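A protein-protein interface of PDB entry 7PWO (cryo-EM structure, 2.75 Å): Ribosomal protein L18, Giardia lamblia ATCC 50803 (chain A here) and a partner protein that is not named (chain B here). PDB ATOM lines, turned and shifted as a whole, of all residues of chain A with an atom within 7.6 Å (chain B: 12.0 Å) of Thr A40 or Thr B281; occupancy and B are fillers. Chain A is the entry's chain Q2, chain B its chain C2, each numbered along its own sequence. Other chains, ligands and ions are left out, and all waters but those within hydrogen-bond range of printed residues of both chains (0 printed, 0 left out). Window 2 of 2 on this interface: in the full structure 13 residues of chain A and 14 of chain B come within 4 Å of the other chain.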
ATOM      1  N   PHE A  33      27.553 -34.467  32.836  1.00  0.00           N
ATOM      2  CA  PHE A  33      27.551 -33.016  32.715  1.00  0.00           C
ATOM      3  C   PHE A  33      28.947 -32.472  32.436  1.00  0.00           C
ATOM      4  O   PHE A  33      29.085 -31.445  31.761  1.00  0.00           O
ATOM      5  CB  PHE A  33      26.944 -32.410  33.968  1.00  0.00           C
ATOM      6  CG  PHE A  33      25.461 -32.242  33.885  1.00  0.00           C
ATOM      7  CD1 PHE A  33      24.902 -31.375  32.974  1.00  0.00           C
ATOM      8  CD2 PHE A  33      24.619 -32.980  34.695  1.00  0.00           C
ATOM      9  CE1 PHE A  33      23.531 -31.235  32.888  1.00  0.00           C
ATOM     10  CE2 PHE A  33      23.250 -32.828  34.609  1.00  0.00           C
ATOM     11  CZ  PHE A  33      22.715 -31.953  33.716  1.00  0.00           C
ATOM     12  N   LYS A  34      29.991 -33.169  32.892  1.00  0.00           N
ATOM     13  CA  LYS A  34      31.352 -32.785  32.537  1.00  0.00           C
ATOM     14  C   LYS A  34      31.588 -32.922  31.035  1.00  0.00           C
ATOM     15  O   LYS A  34      32.233 -32.063  30.417  1.00  0.00           O
ATOM     16  CB  LYS A  34      32.338 -33.638  33.328  1.00  0.00           C
ATOM     17  CG  LYS A  34      33.691 -33.019  33.529  1.00  0.00           C
ATOM     18  CD  LYS A  34      34.668 -34.022  34.090  1.00  0.00           C
ATOM     19  CE  LYS A  34      36.080 -33.653  33.722  1.00  0.00           C
ATOM     20  NZ  LYS A  34      36.218 -33.306  32.282  1.00  0.00           N
ATOM     21  N   VAL A  35      31.052 -33.985  30.424  1.00  0.00           N
ATOM     22  CA  VAL A  35      31.131 -34.130  28.966  1.00  0.00           C
ATOM     23  C   VAL A  35      30.401 -32.989  28.263  1.00  0.00           C
ATOM     24  O   VAL A  35      30.902 -32.411  27.288  1.00  0.00           O
ATOM     25  CB  VAL A  35      30.571 -35.495  28.527  1.00  0.00           C
ATOM     26  CG1 VAL A  35      30.548 -35.587  27.027  1.00  0.00           C
ATOM     27  CG2 VAL A  35      31.417 -36.616  29.084  1.00  0.00           C
ATOM     28  N   VAL A  36      29.188 -32.677  28.720  1.00  0.00           N
ATOM     29  CA  VAL A  36      28.430 -31.602  28.079  1.00  0.00           C
ATOM     30  C   VAL A  36      29.195 -30.286  28.152  1.00  0.00           C
ATOM     31  O   VAL A  36      29.276 -29.551  27.159  1.00  0.00           O
ATOM     32  CB  VAL A  36      27.021 -31.479  28.686  1.00  0.00           C
ATOM     33  CG1 VAL A  36      26.303 -30.296  28.096  1.00  0.00           C
ATOM     34  CG2 VAL A  36      26.218 -32.725  28.378  1.00  0.00           C
ATOM     35  N   TYR A  37      29.770 -29.964  29.319  1.00  0.00           N
ATOM     36  CA  TYR A  37      30.624 -28.780  29.412  1.00  0.00           C
ATOM     37  C   TYR A  37      31.746 -28.836  28.383  1.00  0.00           C
ATOM     38  O   TYR A  37      31.931 -27.898  27.599  1.00  0.00           O
ATOM     39  CB  TYR A  37      31.227 -28.629  30.811  1.00  0.00           C
ATOM     40  CG  TYR A  37      32.119 -27.414  30.872  1.00  0.00           C
ATOM     41  CD1 TYR A  37      31.631 -26.172  30.533  1.00  0.00           C
ATOM     42  CD2 TYR A  37      33.476 -27.528  31.115  1.00  0.00           C
ATOM     43  CE1 TYR A  37      32.426 -25.064  30.522  1.00  0.00           C
ATOM     44  CE2 TYR A  37      34.297 -26.412  31.102  1.00  0.00           C
ATOM     45  CZ  TYR A  37      33.756 -25.180  30.804  1.00  0.00           C
ATOM     46  OH  TYR A  37      34.542 -24.052  30.788  1.00  0.00           O
ATOM     47  N   GLU A  38      32.492 -29.946  28.363  1.00  0.00           N
ATOM     48  CA  GLU A  38      33.626 -30.078  27.455  1.00  0.00           C
ATOM     49  C   GLU A  38      33.230 -29.787  26.019  1.00  0.00           C
ATOM     50  O   GLU A  38      34.010 -29.215  25.253  1.00  0.00           O
ATOM     51  CB  GLU A  38      34.202 -31.487  27.538  1.00  0.00           C
ATOM     52  CG  GLU A  38      35.213 -31.710  28.628  1.00  0.00           C
ATOM     53  CD  GLU A  38      35.648 -33.156  28.700  1.00  0.00           C
ATOM     54  OE1 GLU A  38      36.868 -33.416  28.679  1.00  0.00           O
ATOM     55  OE2 GLU A  38      34.772 -34.041  28.769  1.00  0.00           O
ATOM     56  N   ASN A  39      32.027 -30.189  25.628  1.00  0.00           N
ATOM     57  CA  ASN A  39      31.668 -30.107  24.219  1.00  0.00           C
ATOM     58  C   ASN A  39      30.891 -28.855  23.844  1.00  0.00           C
ATOM     59  O   ASN A  39      30.780 -28.561  22.655  1.00  0.00           O
ATOM     60  CB  ASN A  39      30.878 -31.354  23.806  1.00  0.00           C
ATOM     61  CG  ASN A  39      31.741 -32.595  23.795  1.00  0.00           C
ATOM     62  OD1 ASN A  39      32.918 -32.556  24.135  1.00  0.00           O
ATOM     63  ND2 ASN A  39      31.147 -33.716  23.422  1.00  0.00           N
ATOM     64  N   THR A  40      30.363 -28.102  24.804  1.00  0.00           N
ATOM     65  CA  THR A  40      29.593 -26.918  24.454  1.00  0.00           C
ATOM     66  C   THR A  40      30.099 -25.610  25.040  1.00  0.00           C
ATOM     67  O   THR A  40      29.606 -24.552  24.633  1.00  0.00           O
ATOM     68  CB  THR A  40      28.131 -27.077  24.887  1.00  0.00           C
ATOM     69  OG1 THR A  40      27.363 -26.020  24.308  1.00  0.00           O
ATOM     70  CG2 THR A  40      28.023 -26.949  26.383  1.00  0.00           C
ATOM     71  N   GLY A  41      31.040 -25.630  25.976  1.00  0.00           N
ATOM     72  CA  GLY A  41      31.280 -24.420  26.740  1.00  0.00           C
ATOM     73  C   GLY A  41      30.149 -24.251  27.732  1.00  0.00           C
ATOM     74  O   GLY A  41      29.884 -25.174  28.501  1.00  0.00           O
ATOM     75  N   GLU A  42      29.437 -23.123  27.698  1.00  0.00           N
ATOM     76  CA  GLU A  42      28.269 -22.945  28.559  1.00  0.00           C
ATOM     77  C   GLU A  42      28.607 -23.003  30.044  1.00  0.00           C
ATOM     78  O   GLU A  42      28.510 -24.054  30.696  1.00  0.00           O
ATOM     79  CB  GLU A  42      27.168 -23.933  28.208  1.00  0.00           C
ATOM     80  CG  GLU A  42      26.603 -23.671  26.836  1.00  0.00           C
ATOM     81  CD  GLU A  42      25.872 -22.345  26.765  1.00  0.00           C
ATOM     82  OE1 GLU A  42      25.291 -21.936  27.787  1.00  0.00           O
ATOM     83  OE2 GLU A  42      25.872 -21.711  25.693  1.00  0.00           O
ATOM     84  N   ASP A  43      29.126 -21.882  30.548  1.00  0.00           N
ATOM     85  CA  ASP A  43      29.370 -21.734  31.975  1.00  0.00           C
ATOM     86  C   ASP A  43      28.206 -22.203  32.839  1.00  0.00           C
ATOM     87  O   ASP A  43      28.422 -22.496  34.014  1.00  0.00           O
ATOM     88  CB  ASP A  43      29.702 -20.282  32.319  1.00  0.00           C
ATOM     89  CG  ASP A  43      28.580 -19.337  32.003  1.00  0.00           C
ATOM     90  OD1 ASP A  43      27.717 -19.126  32.875  1.00  0.00           O
ATOM     91  OD2 ASP A  43      28.560 -18.787  30.880  1.00  0.00           O
ATOM     92  N   THR A  45      26.612 -25.113  32.343  1.00  0.00           N
ATOM     93  CA  THR A  45      27.011 -26.491  32.569  1.00  0.00           C
ATOM     94  C   THR A  45      28.283 -26.551  33.407  1.00  0.00           C
ATOM     95  O   THR A  45      28.460 -27.485  34.195  1.00  0.00           O
ATOM     96  CB  THR A  45      27.179 -27.210  31.230  1.00  0.00           C
ATOM     97  OG1 THR A  45      25.939 -27.181  30.518  1.00  0.00           O
ATOM     98  CG2 THR A  45      27.524 -28.662  31.443  1.00  0.00           C
ATOM     99  N   LYS A  46      29.151 -25.537  33.294  1.00  0.00           N
ATOM    100  CA  LYS A  46      30.358 -25.495  34.127  1.00  0.00           C
ATOM    101  C   LYS A  46      30.030 -25.369  35.615  1.00  0.00           C
ATOM    102  O   LYS A  46      30.573 -26.104  36.451  1.00  0.00           O
ATOM    103  CB  LYS A  46      31.258 -24.342  33.687  1.00  0.00           C
ATOM    104  CG  LYS A  46      32.559 -24.240  34.457  1.00  0.00           C
ATOM    105  CD  LYS A  46      33.441 -23.149  33.896  1.00  0.00           C
ATOM    106  CE  LYS A  46      34.675 -22.929  34.754  1.00  0.00           C
ATOM    107  NZ  LYS A  46      35.622 -24.076  34.786  1.00  0.00           N
ATOM    108  N   LYS A 129      16.935 -30.323  28.504  1.00  0.00           N
ATOM    109  CA  LYS A 129      17.761 -29.145  28.274  1.00  0.00           C
ATOM    110  C   LYS A 129      19.088 -29.216  29.026  1.00  0.00           C
ATOM    111  O   LYS A 129      19.146 -28.974  30.236  1.00  0.00           O
ATOM    112  CB  LYS A 129      16.971 -27.879  28.617  1.00  0.00           C
ATOM    113  CG  LYS A 129      16.555 -27.702  30.060  1.00  0.00           C
ATOM    114  CD  LYS A 129      15.823 -26.399  30.202  1.00  0.00           C
ATOM    115  CE  LYS A 129      14.445 -26.414  29.613  1.00  0.00           C
ATOM    116  NZ  LYS A 129      13.767 -25.131  29.917  1.00  0.00           N
ATOM    117  N   PRO A 130      20.184 -29.555  28.344  1.00  0.00           N
ATOM    118  CA  PRO A 130      21.450 -29.793  29.044  1.00  0.00           C
ATOM    119  C   PRO A 130      22.302 -28.561  29.286  1.00  0.00           C
ATOM    120  O   PRO A 130      23.313 -28.669  29.990  1.00  0.00           O
ATOM    121  CB  PRO A 130      22.171 -30.760  28.100  1.00  0.00           C
ATOM    122  CG  PRO A 130      21.667 -30.377  26.734  1.00  0.00           C
ATOM    123  CD  PRO A 130      20.279 -29.837  26.900  1.00  0.00           C
ATOM    124  N   THR A 131      21.938 -27.406  28.741  1.00  0.00           N
ATOM    125  CA  THR A 131      22.750 -26.213  28.887  1.00  0.00           C
ATOM    126  C   THR A 131      22.053 -25.089  29.638  1.00  0.00           C
ATOM    127  O   THR A 131      22.652 -24.023  29.808  1.00  0.00           O
ATOM    128  CB  THR A 131      23.208 -25.710  27.514  1.00  0.00           C
ATOM    129  OG1 THR A 131      22.085 -25.640  26.632  1.00  0.00           O
ATOM    130  CG2 THR A 131      24.261 -26.637  26.941  1.00  0.00           C
ATOM    131  N   ASP A 133      18.979 -23.217  29.274  1.00  0.00           N
ATOM    132  CA  ASP A 133      18.223 -22.105  28.708  1.00  0.00           C
ATOM    133  C   ASP A 133      16.860 -22.051  29.389  1.00  0.00           C
ATOM    134  O   ASP A 133      16.056 -22.975  29.240  1.00  0.00           O
ATOM    135  CB  ASP A 133      18.085 -22.269  27.198  1.00  0.00           C
ATOM    136  CG  ASP A 133      19.407 -22.096  26.460  1.00  0.00           C
ATOM    137  OD1 ASP A 133      20.284 -21.349  26.932  1.00  0.00           O
ATOM    138  OD2 ASP A 133      19.588 -22.749  25.420  1.00  0.00           O
ATOM    139  N   ILE B 272      20.975 -41.093  26.349  1.00  0.00           N
ATOM    140  CA  ILE B 272      20.625 -39.678  26.301  1.00  0.00           C
ATOM    141  C   ILE B 272      21.685 -38.912  25.527  1.00  0.00           C
ATOM    142  O   ILE B 272      21.382 -38.182  24.577  1.00  0.00           O
ATOM    143  CB  ILE B 272      20.455 -39.097  27.713  1.00  0.00           C
ATOM    144  CG1 ILE B 272      19.314 -39.757  28.475  1.00  0.00           C
ATOM    145  CG2 ILE B 272      20.131 -37.642  27.606  1.00  0.00           C
ATOM    146  CD1 ILE B 272      19.306 -39.381  29.932  1.00  0.00           C
ATOM    147  N   LEU B 273      22.953 -39.108  25.896  1.00  0.00           N
ATOM    148  CA  LEU B 273      24.025 -38.307  25.315  1.00  0.00           C
ATOM    149  C   LEU B 273      24.115 -38.494  23.806  1.00  0.00           C
ATOM    150  O   LEU B 273      24.280 -37.520  23.064  1.00  0.00           O
ATOM    151  CB  LEU B 273      25.355 -38.665  25.966  1.00  0.00           C
ATOM    152  CG  LEU B 273      25.690 -37.886  27.232  1.00  0.00           C
ATOM    153  CD1 LEU B 273      27.051 -38.311  27.730  1.00  0.00           C
ATOM    154  CD2 LEU B 273      25.635 -36.397  26.954  1.00  0.00           C
ATOM    155  N   GLN B 274      24.016 -39.735  23.328  1.00  0.00           N
ATOM    156  CA  GLN B 274      24.061 -39.923  21.881  1.00  0.00           C
ATOM    157  C   GLN B 274      22.754 -39.582  21.167  1.00  0.00           C
ATOM    158  O   GLN B 274      22.758 -39.477  19.938  1.00  0.00           O
ATOM    159  CB  GLN B 274      24.534 -41.342  21.557  1.00  0.00           C
ATOM    160  CG  GLN B 274      26.039 -41.555  21.785  1.00  0.00           C
ATOM    161  CD  GLN B 274      26.496 -41.515  23.230  1.00  0.00           C
ATOM    162  OE1 GLN B 274      27.318 -40.673  23.586  1.00  0.00           O
ATOM    163  NE2 GLN B 274      25.969 -42.403  24.067  1.00  0.00           N
ATOM    164  N   SER B 275      21.657 -39.364  21.886  1.00  0.00           N
ATOM    165  CA  SER B 275      20.439 -38.883  21.247  1.00  0.00           C
ATOM    166  C   SER B 275      20.674 -37.522  20.596  1.00  0.00           C
ATOM    167  O   SER B 275      21.680 -36.853  20.829  1.00  0.00           O
ATOM    168  CB  SER B 275      19.303 -38.762  22.259  1.00  0.00           C
ATOM    169  OG  SER B 275      19.517 -37.652  23.111  1.00  0.00           O
ATOM    170  N   ASP B 276      19.690 -37.095  19.798  1.00  0.00           N
ATOM    171  CA  ASP B 276      19.833 -35.901  18.969  1.00  0.00           C
ATOM    172  C   ASP B 276      19.548 -34.604  19.716  1.00  0.00           C
ATOM    173  O   ASP B 276      20.091 -33.557  19.349  1.00  0.00           O
ATOM    174  CB  ASP B 276      18.926 -36.006  17.736  1.00  0.00           C
ATOM    175  CG  ASP B 276      17.452 -35.756  18.053  1.00  0.00           C
ATOM    176  OD1 ASP B 276      17.037 -35.933  19.220  1.00  0.00           O
ATOM    177  OD2 ASP B 276      16.702 -35.384  17.124  1.00  0.00           O
ATOM    178  N   ALA B 277      18.710 -34.635  20.753  1.00  0.00           N
ATOM    179  CA  ALA B 277      18.401 -33.397  21.464  1.00  0.00           C
ATOM    180  C   ALA B 277      19.604 -32.842  22.219  1.00  0.00           C
ATOM    181  O   ALA B 277      19.610 -31.658  22.569  1.00  0.00           O
ATOM    182  CB  ALA B 277      17.234 -33.614  22.420  1.00  0.00           C
ATOM    183  N   VAL B 278      20.621 -33.664  22.471  1.00  0.00           N
ATOM    184  CA  VAL B 278      21.841 -33.221  23.134  1.00  0.00           C
ATOM    185  C   VAL B 278      22.949 -32.944  22.121  1.00  0.00           C
ATOM    186  O   VAL B 278      23.736 -32.013  22.291  1.00  0.00           O
ATOM    187  CB  VAL B 278      22.277 -34.280  24.172  1.00  0.00           C
ATOM    188  CG1 VAL B 278      23.607 -33.915  24.843  1.00  0.00           C
ATOM    189  CG2 VAL B 278      21.182 -34.525  25.185  1.00  0.00           C
ATOM    190  N   GLN B 279      22.999 -33.737  21.048  1.00  0.00           N
ATOM    191  CA  GLN B 279      23.957 -33.515  19.971  1.00  0.00           C
ATOM    192  C   GLN B 279      23.657 -32.237  19.189  1.00  0.00           C
ATOM    193  O   GLN B 279      24.572 -31.642  18.614  1.00  0.00           O
ATOM    194  CB  GLN B 279      23.966 -34.714  19.020  1.00  0.00           C
ATOM    195  CG  GLN B 279      24.429 -36.030  19.636  1.00  0.00           C
ATOM    196  CD  GLN B 279      25.888 -36.003  20.040  1.00  0.00           C
ATOM    197  OE1 GLN B 279      26.725 -35.437  19.342  1.00  0.00           O
ATOM    198  NE2 GLN B 279      26.197 -36.604  21.180  1.00  0.00           N
ATOM    199  N   LYS B 280      22.398 -31.791  19.166  1.00  0.00           N
ATOM    200  CA  LYS B 280      22.050 -30.587  18.419  1.00  0.00           C
ATOM    201  C   LYS B 280      22.684 -29.319  18.980  1.00  0.00           C
ATOM    202  O   LYS B 280      22.629 -28.281  18.312  1.00  0.00           O
ATOM    203  CB  LYS B 280      20.532 -30.373  18.376  1.00  0.00           C
ATOM    204  CG  LYS B 280      19.917 -30.017  19.719  1.00  0.00           C
ATOM    205  CD  LYS B 280      18.495 -29.487  19.571  1.00  0.00           C
ATOM    206  CE  LYS B 280      18.507 -27.975  19.376  1.00  0.00           C
ATOM    207  NZ  LYS B 280      17.236 -27.431  18.830  1.00  0.00           N
ATOM    208  N   THR B 281      23.257 -29.357  20.184  1.00  0.00           N
ATOM    209  CA  THR B 281      23.842 -28.172  20.800  1.00  0.00           C
ATOM    210  C   THR B 281      25.361 -28.228  20.878  1.00  0.00           C
ATOM    211  O   THR B 281      25.959 -27.473  21.648  1.00  0.00           O
ATOM    212  CB  THR B 281      23.276 -27.959  22.202  1.00  0.00           C
ATOM    213  OG1 THR B 281      23.851 -28.916  23.100  1.00  0.00           O
ATOM    214  CG2 THR B 281      21.777 -28.127  22.190  1.00  0.00           C
ATOM    215  N   PHE B 282      26.003 -29.102  20.111  1.00  0.00           N
ATOM    216  CA  PHE B 282      27.453 -29.152  20.174  1.00  0.00           C
ATOM    217  C   PHE B 282      28.068 -28.091  19.258  1.00  0.00           C
ATOM    218  O   PHE B 282      27.383 -27.412  18.491  1.00  0.00           O
ATOM    219  CB  PHE B 282      27.961 -30.553  19.831  1.00  0.00           C
ATOM    220  CG  PHE B 282      27.774 -31.560  20.937  1.00  0.00           C
ATOM    221  CD1 PHE B 282      26.944 -31.297  22.011  1.00  0.00           C
ATOM    222  CD2 PHE B 282      28.428 -32.772  20.897  1.00  0.00           C
ATOM    223  CE1 PHE B 282      26.767 -32.228  23.015  1.00  0.00           C
ATOM    224  CE2 PHE B 282      28.261 -33.703  21.908  1.00  0.00           C
ATOM    225  CZ  PHE B 282      27.432 -33.433  22.962  1.00  0.00           C
ATOM    226  N   VAL B 283      29.380 -27.928  19.377  1.00  0.00           N
ATOM    227  CA  VAL B 283      30.112 -26.885  18.660  1.00  0.00           C
ATOM    228  C   VAL B 283      31.597 -27.235  18.678  1.00  0.00           C
ATOM    229  O   VAL B 283      32.160 -27.522  19.744  1.00  0.00           O
ATOM    230  CB  VAL B 283      29.819 -25.492  19.248  1.00  0.00           C
ATOM    231  CG1 VAL B 283      30.315 -25.364  20.679  1.00  0.00           C
ATOM    232  CG2 VAL B 283      30.441 -24.406  18.377  1.00  0.00           C
ATOM    233  N   PRO B 284      32.256 -27.256  17.519  1.00  0.00           N
ATOM    234  CA  PRO B 284      33.657 -27.690  17.462  1.00  0.00           C
ATOM    235  C   PRO B 284      34.592 -26.738  18.185  1.00  0.00           C
ATOM    236  O   PRO B 284      34.347 -25.532  18.274  1.00  0.00           O
ATOM    237  CB  PRO B 284      33.966 -27.709  15.959  1.00  0.00           C
ATOM    238  CG  PRO B 284      32.645 -27.592  15.264  1.00  0.00           C
ATOM    239  CD  PRO B 284      31.727 -26.891  16.195  1.00  0.00           C
ATOM    240  N   LYS B 285      35.695 -27.299  18.677  1.00  0.00           N
ATOM    241  CA  LYS B 285      36.728 -26.519  19.332  1.00  0.00           C
ATOM    242  C   LYS B 285      37.653 -25.912  18.274  1.00  0.00           C
ATOM    243  O   LYS B 285      37.654 -26.318  17.110  1.00  0.00           O
ATOM    244  CB  LYS B 285      37.562 -27.396  20.270  1.00  0.00           C
ATOM    245  CG  LYS B 285      36.802 -28.117  21.404  1.00  0.00           C
ATOM    246  CD  LYS B 285      36.240 -27.272  22.547  1.00  0.00           C
ATOM    247  CE  LYS B 285      34.774 -26.900  22.280  1.00  0.00           C
ATOM    248  NZ  LYS B 285      34.106 -26.168  23.389  1.00  0.00           N
ATOM    249  N   ARG B 286      38.454 -24.937  18.691  1.00  0.00           N
ATOM    250  CA  ARG B 286      39.543 -24.453  17.849  1.00  0.00           C
ATOM    251  C   ARG B 286      40.551 -25.572  17.599  1.00  0.00           C
ATOM    252  O   ARG B 286      40.693 -26.496  18.401  1.00  0.00           O
ATOM    253  CB  ARG B 286      40.223 -23.242  18.508  1.00  0.00           C
ATOM    254  CG  ARG B 286      41.306 -22.572  17.664  1.00  0.00           C
ATOM    255  CD  ARG B 286      41.901 -21.321  18.333  1.00  0.00           C
ATOM    256  NE  ARG B 286      42.606 -21.625  19.569  1.00  0.00           N
ATOM    257  CZ  ARG B 286      42.191 -21.217  20.760  1.00  0.00           C
ATOM    258  NH1 ARG B 286      41.090 -20.488  20.855  1.00  0.00           N
ATOM    259  NH2 ARG B 286      42.862 -21.540  21.851  1.00  0.00           N
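Of chain B, only Thr B281 (3.3 Å) comes within 4 Å of Thr A40. Thr B281 touches just one residue of chain A: Thr A40. Asn A39 touches just these residues of chain B: Phe B282 and Val B283. No residue of chain B comes within 4 Å of Thr A45. No residue of chain B comes within 4 Å of Pro A130. Of the printed residues of chain B, Val A36 touches Leu B273 (3.98 Å). Of the printed residues of chain A, Val B283 touches Asn A39 (3.4 Å). Printed residues of chain A within 4 Å of Leu B273: Val A36. Of the printed residues of chain A, Lys B285 touches Glu A38. Of the printed residues of chain A, Phe B282 touches Asn A39. Ala B277 touches none of the printed residues of chain A.
Among the printed residues, merely in contact across the chains: Val A36 with Leu B273, Glu A38 with Lys B285 and Asn A39 with Phe B282.
The backbone carbonyl oxygen (O) of Thr B281 is in hydrogen-bond range of the side-chain hydroxyl (OG1) of Thr A40, at 3.3 Å. The backbone carbonyl oxygen of Asn A39 lies close to the backbone carbonyl oxygen of Val B283, 3.4 Å away.
Hydrophobic or aromatic side chains of chain A within 4 Å of the printed part of chain B: Val A36. Printed residues of chain B that touch a printed residue of chain A: Leu B273, Thr B281, Phe B282, Val B283 and Lys B285. Among the printed residues, 5 pairs touch across the chains. Among the printed residues, no Asp or Glu carboxylate lies within 4 Å of a Lys or Arg side-chain nitrogen of the other chain.
NE2 of Gln B279 lies within hydrogen-bond range of O of Leu B273 (2.8 Å). The side-chain hydroxyl of Thr B281 is in hydrogen-bond range of the backbone carbonyl oxygen of Val B278 (3.2 Å). The side-chain carboxylate (OE1) of Glu A38 is in salt-bridge range of the side-chain amino group (NZ) of Lys A34 (3.7 Å).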
